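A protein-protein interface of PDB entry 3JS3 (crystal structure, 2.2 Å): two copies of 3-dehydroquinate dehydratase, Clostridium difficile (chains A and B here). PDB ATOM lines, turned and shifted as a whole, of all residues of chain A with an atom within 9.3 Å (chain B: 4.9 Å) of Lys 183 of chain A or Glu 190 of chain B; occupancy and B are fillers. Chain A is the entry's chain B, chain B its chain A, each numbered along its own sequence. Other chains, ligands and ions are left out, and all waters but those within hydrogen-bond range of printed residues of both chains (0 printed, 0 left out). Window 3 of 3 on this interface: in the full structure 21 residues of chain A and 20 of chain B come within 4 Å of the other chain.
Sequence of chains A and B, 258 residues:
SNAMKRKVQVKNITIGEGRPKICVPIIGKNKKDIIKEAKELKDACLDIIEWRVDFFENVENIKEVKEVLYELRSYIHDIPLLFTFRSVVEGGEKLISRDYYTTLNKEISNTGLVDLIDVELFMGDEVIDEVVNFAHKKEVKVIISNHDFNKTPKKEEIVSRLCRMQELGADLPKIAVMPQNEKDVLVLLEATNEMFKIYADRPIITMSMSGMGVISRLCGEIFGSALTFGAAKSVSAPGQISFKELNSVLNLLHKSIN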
ATOM      1  N   THR A 152     -26.582 -28.185 -12.409  1.00  0.00           N
ATOM      2  CA  THR A 152     -26.215 -26.803 -12.289  1.00  0.00           C
ATOM      3  C   THR A 152     -27.001 -26.283 -11.089  1.00  0.00           C
ATOM      4  O   THR A 152     -28.222 -26.238 -11.134  1.00  0.00           O
ATOM      5  CB  THR A 152     -26.606 -26.001 -13.549  1.00  0.00           C
ATOM      6  OG1 THR A 152     -25.896 -26.502 -14.689  1.00  0.00           O
ATOM      7  CG2 THR A 152     -26.288 -24.543 -13.380  1.00  0.00           C
ATOM      8  N   PRO A 153     -26.311 -25.941  -9.991  1.00  0.00           N
ATOM      9  CA  PRO A 153     -27.023 -25.375  -8.858  1.00  0.00           C
ATOM     10  C   PRO A 153     -27.671 -24.049  -9.257  1.00  0.00           C
ATOM     11  O   PRO A 153     -27.276 -23.457 -10.282  1.00  0.00           O
ATOM     12  CB  PRO A 153     -25.911 -25.122  -7.830  1.00  0.00           C
ATOM     13  CG  PRO A 153     -24.767 -25.961  -8.264  1.00  0.00           C
ATOM     14  CD  PRO A 153     -24.869 -26.071  -9.738  1.00  0.00           C
ATOM     15  N   LYS A 154     -28.636 -23.587  -8.456  1.00  0.00           N
ATOM     16  CA  LYS A 154     -29.331 -22.332  -8.709  1.00  0.00           C
ATOM     17  C   LYS A 154     -28.295 -21.233  -8.701  1.00  0.00           C
ATOM     18  O   LYS A 154     -27.274 -21.358  -8.052  1.00  0.00           O
ATOM     19  CB  LYS A 154     -30.336 -21.989  -7.596  1.00  0.00           C
ATOM     20  CG  LYS A 154     -31.324 -23.053  -7.153  1.00  0.00           C
ATOM     21  CD  LYS A 154     -32.590 -23.186  -7.983  1.00  0.00           C
ATOM     22  CE  LYS A 154     -33.616 -24.002  -7.158  1.00  0.00           C
ATOM     23  NZ  LYS A 154     -34.898 -24.224  -7.862  1.00  0.00           N
ATOM     24  N   LYS A 155     -28.590 -20.137  -9.386  1.00  0.00           N
ATOM     25  CA  LYS A 155     -27.684 -18.992  -9.476  1.00  0.00           C
ATOM     26  C   LYS A 155     -27.086 -18.577  -8.131  1.00  0.00           C
ATOM     27  O   LYS A 155     -25.865 -18.432  -8.006  1.00  0.00           O
ATOM     28  CB  LYS A 155     -28.442 -17.807 -10.081  1.00  0.00           C
ATOM     29  CG  LYS A 155     -27.673 -16.495 -10.153  1.00  0.00           C
ATOM     30  CD  LYS A 155     -28.575 -15.373 -10.674  1.00  0.00           C
ATOM     31  CE  LYS A 155     -27.873 -14.020 -10.654  1.00  0.00           C
ATOM     32  NZ  LYS A 155     -28.806 -12.897 -11.003  1.00  0.00           N
ATOM     33  N   ILE A 158     -24.242 -20.699  -6.773  1.00  0.00           N
ATOM     34  CA  ILE A 158     -23.002 -20.566  -7.540  1.00  0.00           C
ATOM     35  C   ILE A 158     -22.276 -19.314  -7.041  1.00  0.00           C
ATOM     36  O   ILE A 158     -21.087 -19.340  -6.760  1.00  0.00           O
ATOM     37  CB  ILE A 158     -23.249 -20.442  -9.080  1.00  0.00           C
ATOM     38  CG1 ILE A 158     -23.946 -21.686  -9.634  1.00  0.00           C
ATOM     39  CG2 ILE A 158     -21.951 -20.239  -9.809  1.00  0.00           C
ATOM     40  CD1 ILE A 158     -24.325 -21.576 -11.097  1.00  0.00           C
ATOM     41  N   VAL A 177     -19.862 -26.480 -13.789  1.00  0.00           N
ATOM     42  CA  VAL A 177     -21.115 -27.167 -13.514  1.00  0.00           C
ATOM     43  C   VAL A 177     -21.630 -27.842 -14.778  1.00  0.00           C
ATOM     44  O   VAL A 177     -21.187 -27.537 -15.875  1.00  0.00           O
ATOM     45  CB  VAL A 177     -22.150 -26.181 -12.985  1.00  0.00           C
ATOM     46  CG1 VAL A 177     -21.725 -25.679 -11.611  1.00  0.00           C
ATOM     47  CG2 VAL A 177     -22.350 -24.996 -13.985  1.00  0.00           C
ATOM     48  N   MET A 178     -22.556 -28.767 -14.609  1.00  0.00           N
ATOM     49  CA  MET A 178     -23.109 -29.525 -15.706  1.00  0.00           C
ATOM     50  C   MET A 178     -24.534 -29.089 -15.984  1.00  0.00           C
ATOM     51  O   MET A 178     -25.389 -29.124 -15.088  1.00  0.00           O
ATOM     52  CB  MET A 178     -23.116 -31.017 -15.362  1.00  0.00           C
ATOM     53  CG  MET A 178     -23.551 -31.894 -16.524  1.00  0.00           C
ATOM     54  SD  MET A 178     -22.373 -31.813 -17.894  1.00  0.00           S
ATOM     55  CE  MET A 178     -21.046 -32.861 -17.299  1.00  0.00           C
ATOM     56  N   PRO A 179     -24.806 -28.668 -17.231  1.00  0.00           N
ATOM     57  CA  PRO A 179     -26.169 -28.280 -17.543  1.00  0.00           C
ATOM     58  C   PRO A 179     -26.991 -29.496 -17.852  1.00  0.00           C
ATOM     59  O   PRO A 179     -26.468 -30.429 -18.425  1.00  0.00           O
ATOM     60  CB  PRO A 179     -26.007 -27.433 -18.810  1.00  0.00           C
ATOM     61  CG  PRO A 179     -24.797 -28.037 -19.496  1.00  0.00           C
ATOM     62  CD  PRO A 179     -23.898 -28.516 -18.384  1.00  0.00           C
ATOM     63  N   GLN A 180     -28.247 -29.507 -17.430  1.00  0.00           N
ATOM     64  CA  GLN A 180     -29.174 -30.588 -17.778  1.00  0.00           C
ATOM     65  C   GLN A 180     -30.186 -30.072 -18.817  1.00  0.00           C
ATOM     66  O   GLN A 180     -31.035 -30.819 -19.299  1.00  0.00           O
ATOM     67  CB  GLN A 180     -29.908 -31.099 -16.551  1.00  0.00           C
ATOM     68  CG  GLN A 180     -29.062 -31.909 -15.609  1.00  0.00           C
ATOM     69  CD  GLN A 180     -29.865 -32.388 -14.428  1.00  0.00           C
ATOM     70  OE1 GLN A 180     -30.564 -31.609 -13.788  1.00  0.00           O
ATOM     71  NE2 GLN A 180     -29.769 -33.674 -14.129  1.00  0.00           N
ATOM     72  N   ASN A 181     -30.090 -28.780 -19.128  1.00  0.00           N
ATOM     73  CA  ASN A 181     -30.935 -28.126 -20.112  1.00  0.00           C
ATOM     74  C   ASN A 181     -30.245 -26.853 -20.531  1.00  0.00           C
ATOM     75  O   ASN A 181     -29.272 -26.436 -19.911  1.00  0.00           O
ATOM     76  CB  ASN A 181     -32.345 -27.834 -19.573  1.00  0.00           C
ATOM     77  CG  ASN A 181     -32.345 -26.953 -18.327  1.00  0.00           C
ATOM     78  OD1 ASN A 181     -31.621 -25.958 -18.237  1.00  0.00           O
ATOM     79  ND2 ASN A 181     -33.201 -27.299 -17.373  1.00  0.00           N
ATOM     80  N   GLU A 182     -30.779 -26.220 -21.562  1.00  0.00           N
ATOM     81  CA  GLU A 182     -30.200 -25.018 -22.097  1.00  0.00           C
ATOM     82  C   GLU A 182     -30.267 -23.888 -21.095  1.00  0.00           C
ATOM     83  O   GLU A 182     -29.327 -23.103 -20.964  1.00  0.00           O
ATOM     84  CB  GLU A 182     -30.891 -24.643 -23.401  1.00  0.00           C
ATOM     85  CG  GLU A 182     -30.803 -25.732 -24.516  1.00  0.00           C
ATOM     86  CD  GLU A 182     -31.822 -26.843 -24.364  1.00  0.00           C
ATOM     87  OE1 GLU A 182     -32.635 -26.782 -23.412  1.00  0.00           O
ATOM     88  OE2 GLU A 182     -31.829 -27.771 -25.201  1.00  0.00           O
ATOM     89  N   LYS A 183     -31.380 -23.806 -20.379  1.00  0.00           N
ATOM     90  CA  LYS A 183     -31.547 -22.778 -19.364  1.00  0.00           C
ATOM     91  C   LYS A 183     -30.414 -22.836 -18.314  1.00  0.00           C
ATOM     92  O   LYS A 183     -29.894 -21.802 -17.903  1.00  0.00           O
ATOM     93  CB  LYS A 183     -32.932 -22.891 -18.744  1.00  0.00           C
ATOM     94  CG  LYS A 183     -33.219 -21.909 -17.645  1.00  0.00           C
ATOM     95  CD  LYS A 183     -33.069 -20.477 -18.090  1.00  0.00           C
ATOM     96  CE  LYS A 183     -33.425 -19.546 -16.944  1.00  0.00           C
ATOM     97  NZ  LYS A 183     -34.813 -19.823 -16.470  1.00  0.00           N
ATOM     98  N   ASP A 184     -30.013 -24.034 -17.905  1.00  0.00           N
ATOM     99  CA  ASP A 184     -28.886 -24.181 -16.971  1.00  0.00           C
ATOM    100  C   ASP A 184     -27.611 -23.508 -17.495  1.00  0.00           C
ATOM    101  O   ASP A 184     -26.781 -23.060 -16.723  1.00  0.00           O
ATOM    102  CB  ASP A 184     -28.571 -25.655 -16.690  1.00  0.00           C
ATOM    103  CG  ASP A 184     -29.567 -26.319 -15.775  1.00  0.00           C
ATOM    104  OD1 ASP A 184     -30.451 -25.621 -15.214  1.00  0.00           O
ATOM    105  OD2 ASP A 184     -29.449 -27.560 -15.608  1.00  0.00           O
ATOM    106  N   VAL A 185     -27.447 -23.421 -18.796  1.00  0.00           N
ATOM    107  CA  VAL A 185     -26.265 -22.772 -19.336  1.00  0.00           C
ATOM    108  C   VAL A 185     -26.342 -21.282 -19.098  1.00  0.00           C
ATOM    109  O   VAL A 185     -25.328 -20.630 -18.782  1.00  0.00           O
ATOM    110  CB  VAL A 185     -26.081 -23.049 -20.845  1.00  0.00           C
ATOM    111  CG1 VAL A 185     -24.822 -22.344 -21.366  1.00  0.00           C
ATOM    112  CG2 VAL A 185     -26.004 -24.563 -21.096  1.00  0.00           C
ATOM    113  N   LEU A 186     -27.550 -20.744 -19.202  1.00  0.00           N
ATOM    114  CA  LEU A 186     -27.766 -19.307 -18.993  1.00  0.00           C
ATOM    115  C   LEU A 186     -27.641 -18.975 -17.505  1.00  0.00           C
ATOM    116  O   LEU A 186     -27.197 -17.889 -17.142  1.00  0.00           O
ATOM    117  CB  LEU A 186     -29.124 -18.875 -19.543  1.00  0.00           C
ATOM    118  CG  LEU A 186     -29.332 -19.210 -21.034  1.00  0.00           C
ATOM    119  CD1 LEU A 186     -30.779 -18.962 -21.509  1.00  0.00           C
ATOM    120  CD2 LEU A 186     -28.338 -18.456 -21.870  1.00  0.00           C
ATOM    121  N   VAL A 187     -28.012 -19.923 -16.648  1.00  0.00           N
ATOM    122  CA  VAL A 187     -27.880 -19.722 -15.202  1.00  0.00           C
ATOM    123  C   VAL A 187     -26.397 -19.540 -14.867  1.00  0.00           C
ATOM    124  O   VAL A 187     -26.035 -18.635 -14.142  1.00  0.00           O
ATOM    125  CB  VAL A 187     -28.522 -20.883 -14.384  1.00  0.00           C
ATOM    126  CG1 VAL A 187     -28.234 -20.721 -12.888  1.00  0.00           C
ATOM    127  CG2 VAL A 187     -30.040 -20.941 -14.628  1.00  0.00           C
ATOM    128  N   LEU A 188     -25.536 -20.375 -15.441  1.00  0.00           N
ATOM    129  CA  LEU A 188     -24.106 -20.268 -15.195  1.00  0.00           C
ATOM    130  C   LEU A 188     -23.612 -18.902 -15.618  1.00  0.00           C
ATOM    131  O   LEU A 188     -22.905 -18.209 -14.867  1.00  0.00           O
ATOM    132  CB  LEU A 188     -23.363 -21.390 -15.918  1.00  0.00           C
ATOM    133  CG  LEU A 188     -21.840 -21.564 -15.809  1.00  0.00           C
ATOM    134  CD1 LEU A 188     -21.101 -20.645 -16.714  1.00  0.00           C
ATOM    135  CD2 LEU A 188     -21.349 -21.440 -14.352  1.00  0.00           C
ATOM    136  N   LEU A 189     -24.011 -18.471 -16.802  1.00  0.00           N
ATOM    137  CA  LEU A 189     -23.565 -17.184 -17.290  1.00  0.00           C
ATOM    138  C   LEU A 189     -24.097 -16.047 -16.436  1.00  0.00           C
ATOM    139  O   LEU A 189     -23.404 -15.072 -16.182  1.00  0.00           O
ATOM    140  CB  LEU A 189     -23.968 -16.990 -18.748  1.00  0.00           C
ATOM    141  CG  LEU A 189     -23.264 -17.904 -19.766  1.00  0.00           C
ATOM    142  CD1 LEU A 189     -23.837 -17.683 -21.147  1.00  0.00           C
ATOM    143  CD2 LEU A 189     -21.741 -17.658 -19.752  1.00  0.00           C
ATOM    144  N   GLU A 190     -25.336 -16.172 -15.993  1.00  0.00           N
ATOM    145  CA  GLU A 190     -25.954 -15.130 -15.191  1.00  0.00           C
ATOM    146  C   GLU A 190     -25.235 -14.993 -13.841  1.00  0.00           C
ATOM    147  O   GLU A 190     -24.912 -13.880 -13.404  1.00  0.00           O
ATOM    148  CB  GLU A 190     -27.428 -15.459 -15.020  1.00  0.00           C
ATOM    149  CG  GLU A 190     -28.252 -14.371 -14.447  1.00  0.00           C
ATOM    150  CD  GLU A 190     -29.693 -14.788 -14.310  1.00  0.00           C
ATOM    151  OE1 GLU A 190     -30.470 -14.029 -13.708  1.00  0.00           O
ATOM    152  OE2 GLU A 190     -30.045 -15.887 -14.807  1.00  0.00           O
ATOM    153  N   ALA A 191     -24.963 -16.135 -13.209  1.00  0.00           N
ATOM    154  CA  ALA A 191     -24.269 -16.181 -11.928  1.00  0.00           C
ATOM    155  C   ALA A 191     -22.875 -15.601 -12.089  1.00  0.00           C
ATOM    156  O   ALA A 191     -22.396 -14.825 -11.239  1.00  0.00           O
ATOM    157  CB  ALA A 191     -24.190 -17.613 -11.430  1.00  0.00           C
ATOM    158  N   SER A 208     -19.768 -23.970 -18.022  1.00  0.00           N
ATOM    159  CA  SER A 208     -20.859 -24.912 -18.065  1.00  0.00           C
ATOM    160  C   SER A 208     -20.286 -26.009 -18.939  1.00  0.00           C
ATOM    161  O   SER A 208     -19.899 -25.734 -20.081  1.00  0.00           O
ATOM    162  CB  SER A 208     -22.091 -24.276 -18.711  1.00  0.00           C
ATOM    163  OG  SER A 208     -23.147 -25.206 -18.774  1.00  0.00           O
ATOM    164  N   MET A 212     -23.375 -28.734 -24.853  1.00  0.00           N
ATOM    165  CA  MET A 212     -24.427 -27.764 -24.599  1.00  0.00           C
ATOM    166  C   MET A 212     -23.919 -26.505 -23.903  1.00  0.00           C
ATOM    167  O   MET A 212     -24.465 -25.405 -24.107  1.00  0.00           O
ATOM    168  CB  MET A 212     -25.541 -28.415 -23.746  1.00  0.00           C
ATOM    169  CG  MET A 212     -26.716 -27.520 -23.557  1.00  0.00           C
ATOM    170  SD  MET A 212     -28.109 -28.276 -22.712  1.00  0.00           S
ATOM    171  CE  MET A 212     -28.632 -29.528 -23.879  1.00  0.00           C
ATOM    172  N   LYS B 155     -38.540 -11.408 -21.435  1.00  0.00           N
ATOM    173  CA  LYS B 155     -38.663 -12.658 -22.207  1.00  0.00           C
ATOM    174  C   LYS B 155     -40.092 -12.934 -22.682  1.00  0.00           C
ATOM    175  O   LYS B 155     -40.324 -13.270 -23.855  1.00  0.00           O
ATOM    176  CB  LYS B 155     -38.069 -13.897 -21.486  1.00  0.00           C
ATOM    177  CG  LYS B 155     -38.961 -14.670 -20.552  1.00  0.00           C
ATOM    178  CD  LYS B 155     -38.243 -15.923 -20.070  1.00  0.00           C
ATOM    179  CE  LYS B 155     -38.995 -16.666 -18.936  1.00  0.00           C
ATOM    180  NZ  LYS B 155     -40.292 -17.275 -19.356  1.00  0.00           N
ATOM    181  N   LYS B 183     -27.167  -9.245 -18.804  1.00  0.00           N
ATOM    182  CA  LYS B 183     -28.346 -10.031 -18.526  1.00  0.00           C
ATOM    183  C   LYS B 183     -29.392  -9.953 -19.664  1.00  0.00           C
ATOM    184  O   LYS B 183     -30.089 -10.919 -19.924  1.00  0.00           O
ATOM    185  CB  LYS B 183     -28.942  -9.580 -17.186  1.00  0.00           C
ATOM    186  CG  LYS B 183     -30.258 -10.258 -16.789  1.00  0.00           C
ATOM    187  CD  LYS B 183     -30.195 -11.782 -16.897  1.00  0.00           C
ATOM    188  CE  LYS B 183     -31.534 -12.428 -16.539  1.00  0.00           C
ATOM    189  NZ  LYS B 183     -31.540 -13.874 -16.923  1.00  0.00           N
ATOM    190  N   LEU B 186     -28.853 -12.592 -22.108  1.00  0.00           N
ATOM    191  CA  LEU B 186     -29.322 -13.902 -21.653  1.00  0.00           C
ATOM    192  C   LEU B 186     -30.857 -13.959 -21.727  1.00  0.00           C
ATOM    193  O   LEU B 186     -31.434 -15.014 -22.029  1.00  0.00           O
ATOM    194  CB  LEU B 186     -28.845 -14.179 -20.231  1.00  0.00           C
ATOM    195  CG  LEU B 186     -27.324 -14.118 -20.005  1.00  0.00           C
ATOM    196  CD1 LEU B 186     -27.001 -14.279 -18.521  1.00  0.00           C
ATOM    197  CD2 LEU B 186     -26.606 -15.181 -20.824  1.00  0.00           C
ATOM    198  N   VAL B 187     -31.513 -12.840 -21.446  1.00  0.00           N
ATOM    199  CA  VAL B 187     -32.962 -12.788 -21.574  1.00  0.00           C
ATOM    200  C   VAL B 187     -33.362 -13.169 -23.032  1.00  0.00           C
ATOM    201  O   VAL B 187     -34.267 -13.972 -23.215  1.00  0.00           O
ATOM    202  CB  VAL B 187     -33.532 -11.412 -21.194  1.00  0.00           C
ATOM    203  CG1 VAL B 187     -35.036 -11.369 -21.433  1.00  0.00           C
ATOM    204  CG2 VAL B 187     -33.230 -11.078 -19.711  1.00  0.00           C
ATOM    205  N   LEU B 188     -32.667 -12.611 -24.035  1.00  0.00           N
ATOM    206  CA  LEU B 188     -32.908 -12.912 -25.468  1.00  0.00           C
ATOM    207  C   LEU B 188     -32.715 -14.397 -25.748  1.00  0.00           C
ATOM    208  O   LEU B 188     -33.525 -15.024 -26.402  1.00  0.00           O
ATOM    209  CB  LEU B 188     -31.976 -12.078 -26.362  1.00  0.00           C
ATOM    210  CG  LEU B 188     -32.013 -12.212 -27.893  1.00  0.00           C
ATOM    211  CD1 LEU B 188     -31.251 -13.439 -28.436  1.00  0.00           C
ATOM    212  CD2 LEU B 188     -33.439 -12.173 -28.447  1.00  0.00           C
ATOM    213  N   LEU B 189     -31.620 -14.950 -25.266  1.00  0.00           N
ATOM    214  CA  LEU B 189     -31.365 -16.368 -25.427  1.00  0.00           C
ATOM    215  C   LEU B 189     -32.437 -17.197 -24.718  1.00  0.00           C
ATOM    216  O   LEU B 189     -32.913 -18.184 -25.250  1.00  0.00           O
ATOM    217  CB  LEU B 189     -29.983 -16.732 -24.908  1.00  0.00           C
ATOM    218  CG  LEU B 189     -28.826 -16.158 -25.701  1.00  0.00           C
ATOM    219  CD1 LEU B 189     -27.532 -16.598 -25.077  1.00  0.00           C
ATOM    220  CD2 LEU B 189     -28.899 -16.616 -27.187  1.00  0.00           C
ATOM    221  N   GLU B 190     -32.812 -16.783 -23.514  1.00  0.00           N
ATOM    222  CA  GLU B 190     -33.829 -17.475 -22.764  1.00  0.00           C
ATOM    223  C   GLU B 190     -35.165 -17.517 -23.519  1.00  0.00           C
ATOM    224  O   GLU B 190     -35.828 -18.559 -23.572  1.00  0.00           O
ATOM    225  CB  GLU B 190     -34.022 -16.789 -21.410  1.00  0.00           C
ATOM    226  CG  GLU B 190     -35.023 -17.492 -20.525  1.00  0.00           C
ATOM    227  CD  GLU B 190     -35.050 -16.950 -19.103  1.00  0.00           C
ATOM    228  OE1 GLU B 190     -35.582 -17.664 -18.219  1.00  0.00           O
ATOM    229  OE2 GLU B 190     -34.539 -15.823 -18.864  1.00  0.00           O
ATOM    230  N   ALA B 191     -35.574 -16.377 -24.067  1.00  0.00           N
ATOM    231  CA  ALA B 191     -36.823 -16.295 -24.794  1.00  0.00           C
ATOM    232  C   ALA B 191     -36.745 -17.136 -26.062  1.00  0.00           C
ATOM    233  O   ALA B 191     -37.716 -17.781 -26.431  1.00  0.00           O
ATOM    234  CB  ALA B 191     -37.166 -14.834 -25.131  1.00  0.00           C
ATOM    235  N   THR B 192     -35.582 -17.124 -26.709  1.00  0.00           N
ATOM    236  CA  THR B 192     -35.348 -17.888 -27.938  1.00  0.00           C
ATOM    237  C   THR B 192     -35.549 -19.399 -27.704  1.00  0.00           C
ATOM    238  O   THR B 192     -36.249 -20.068 -28.464  1.00  0.00           O
ATOM    239  CB  THR B 192     -33.928 -17.609 -28.474  1.00  0.00           C
ATOM    240  OG1 THR B 192     -33.835 -16.232 -28.886  1.00  0.00           O
ATOM    241  CG2 THR B 192     -33.577 -18.523 -29.645  1.00  0.00           C
ATOM    242  N   ASN B 193     -34.971 -19.925 -26.628  1.00  0.00           N
ATOM    243  CA  ASN B 193     -35.085 -21.349 -26.372  1.00  0.00           C
ATOM    244  C   ASN B 193     -36.496 -21.766 -25.873  1.00  0.00           C
ATOM    245  O   ASN B 193     -36.978 -22.859 -26.174  1.00  0.00           O
ATOM    246  CB  ASN B 193     -34.025 -21.816 -25.386  1.00  0.00           C
ATOM    247  CG  ASN B 193     -33.870 -23.317 -25.396  1.00  0.00           C
ATOM    248  OD1 ASN B 193     -33.972 -23.973 -24.366  1.00  0.00           O
ATOM    249  ND2 ASN B 193     -33.644 -23.874 -26.584  1.00  0.00           N
ATOM    250  N   GLU B 194     -37.130 -20.906 -25.087  1.00  0.00           N
ATOM    251  CA  GLU B 194     -38.477 -21.172 -24.619  1.00  0.00           C
ATOM    252  C   GLU B 194     -39.362 -21.222 -25.865  1.00  0.00           C
ATOM    253  O   GLU B 194     -40.188 -22.112 -26.021  1.00  0.00           O
ATOM    254  CB  GLU B 194     -38.912 -20.080 -23.656  1.00  0.00           C
ATOM    255  CG  GLU B 194     -40.306 -20.208 -23.146  1.00  0.00           C
ATOM    256  CD  GLU B 194     -40.566 -19.319 -21.942  1.00  0.00           C
ATOM    257  OE1 GLU B 194     -39.661 -19.216 -21.068  1.00  0.00           O
ATOM    258  OE2 GLU B 194     -41.689 -18.760 -21.852  1.00  0.00           O
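Leu 186 of chain A touches Leu 186 of chain B. Leu 186 of chain A touches Leu 189 of chain B. Leu 186 of chain A touches Glu 190 of chain B (CD1 to N, 3.6 Å). CD1 of Leu 189 of chain A touches CD2 of Leu 186 of chain B, 3.7 Å away. Glu 190 of chain A touches Leu 186 of chain B.
The side-chain carboxylate (OE2) of Glu 190 of chain A is in salt-bridge range of the side-chain amino group (NZ) of Lys 183 of chain B. OE1 of Glu 182 of chain A lies close to OD1 of Asn 193 of chain B, at 3.3 Å. The side-chain carboxylate (OE1) of Glu 190 of chain B is in salt-bridge range of the side-chain amino group (NZ) of Lys 183 of chain A.
Lys 183 of chain A touches Glu 190 of chain B, and with the chains exchanged Glu 190 of chain A touches Lys 183 of chain B. Leu 186 of chain A touches its own counterpart, Leu 186 of chain B. Leu 186 of chain A touches Leu 189 of chain B, and with the chains exchanged Leu 189 of chain A touches Leu 186 of chain B. Leu 186 of chain A touches Glu 190 of chain B, and with the chains exchanged Glu 190 of chain A touches Leu 186 of chain B. Of the 8 pairs that touch across the chains among the printed residues, 7 have their exchanged pair printed and touching as well.
The side-chain amino group (NZ) of Lys 155 of chain A lies within salt-bridge range of the side-chain carboxylate (OE1) of Glu 190 of chain A. The backbone NH (N) of Lys 183 of chain A lies within hydrogen-bond range of the side-chain amide oxygen (OD1) of Asn 181 of chain A, 3.0 Å away. The side-chain sulfur (SD) of Met 212 of chain A sits at hydrogen-bond distance from the backbone NH (N) of Glu 182 of chain A (3.6 Å).
Of the 22 printed residues of chain A, 5 touch a printed residue of chain B. Hydrophobic or aromatic side chains of chain A that line the printed part of chain B: Leu 186 and Leu 189. Along chain A the printed residues that touch a printed residue of chain B span positions 182 to 190. Hydrophobic or aromatic side chains of chain B within 4 Å of the printed part of chain A: Leu 186 and Leu 189. Among the printed residues, Asp or Glu carboxylates within 4 Å of a Lys or Arg side-chain nitrogen of the other chain: Lys 183 of chain A with Glu 190 of chain B and Glu 190 of chain A with Lys 183 of chain B.
Thr 152 of chain A touches none of the printed residues of chain B. Lys 155 of chain A touches none of the printed residues of chain B. Lys 183 of chain A touches one residue of chain B. Of the printed residues of chain B, Leu 186 of chain A touches Leu 186 (3.8 Å), Leu 189 (3.8 Å) and Glu 190 (3.6 Å). Of the printed residues of chain B, Glu 190 of chain A touches Lys 183 (3.3 Å) and Leu 186 (3.6 Å). Of the printed residues of chain A, Lys 183 of chain B touches Glu 190. No residue of chain A comes within 4 Å of Val 187 of chain B. Glu 190 of chain B touches just these residues of chain A: Lys 183 (2.9 Å) and Leu 186 (3.6 Å). No residue of chain A comes within 4 Å of Ala 191 of chain B.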
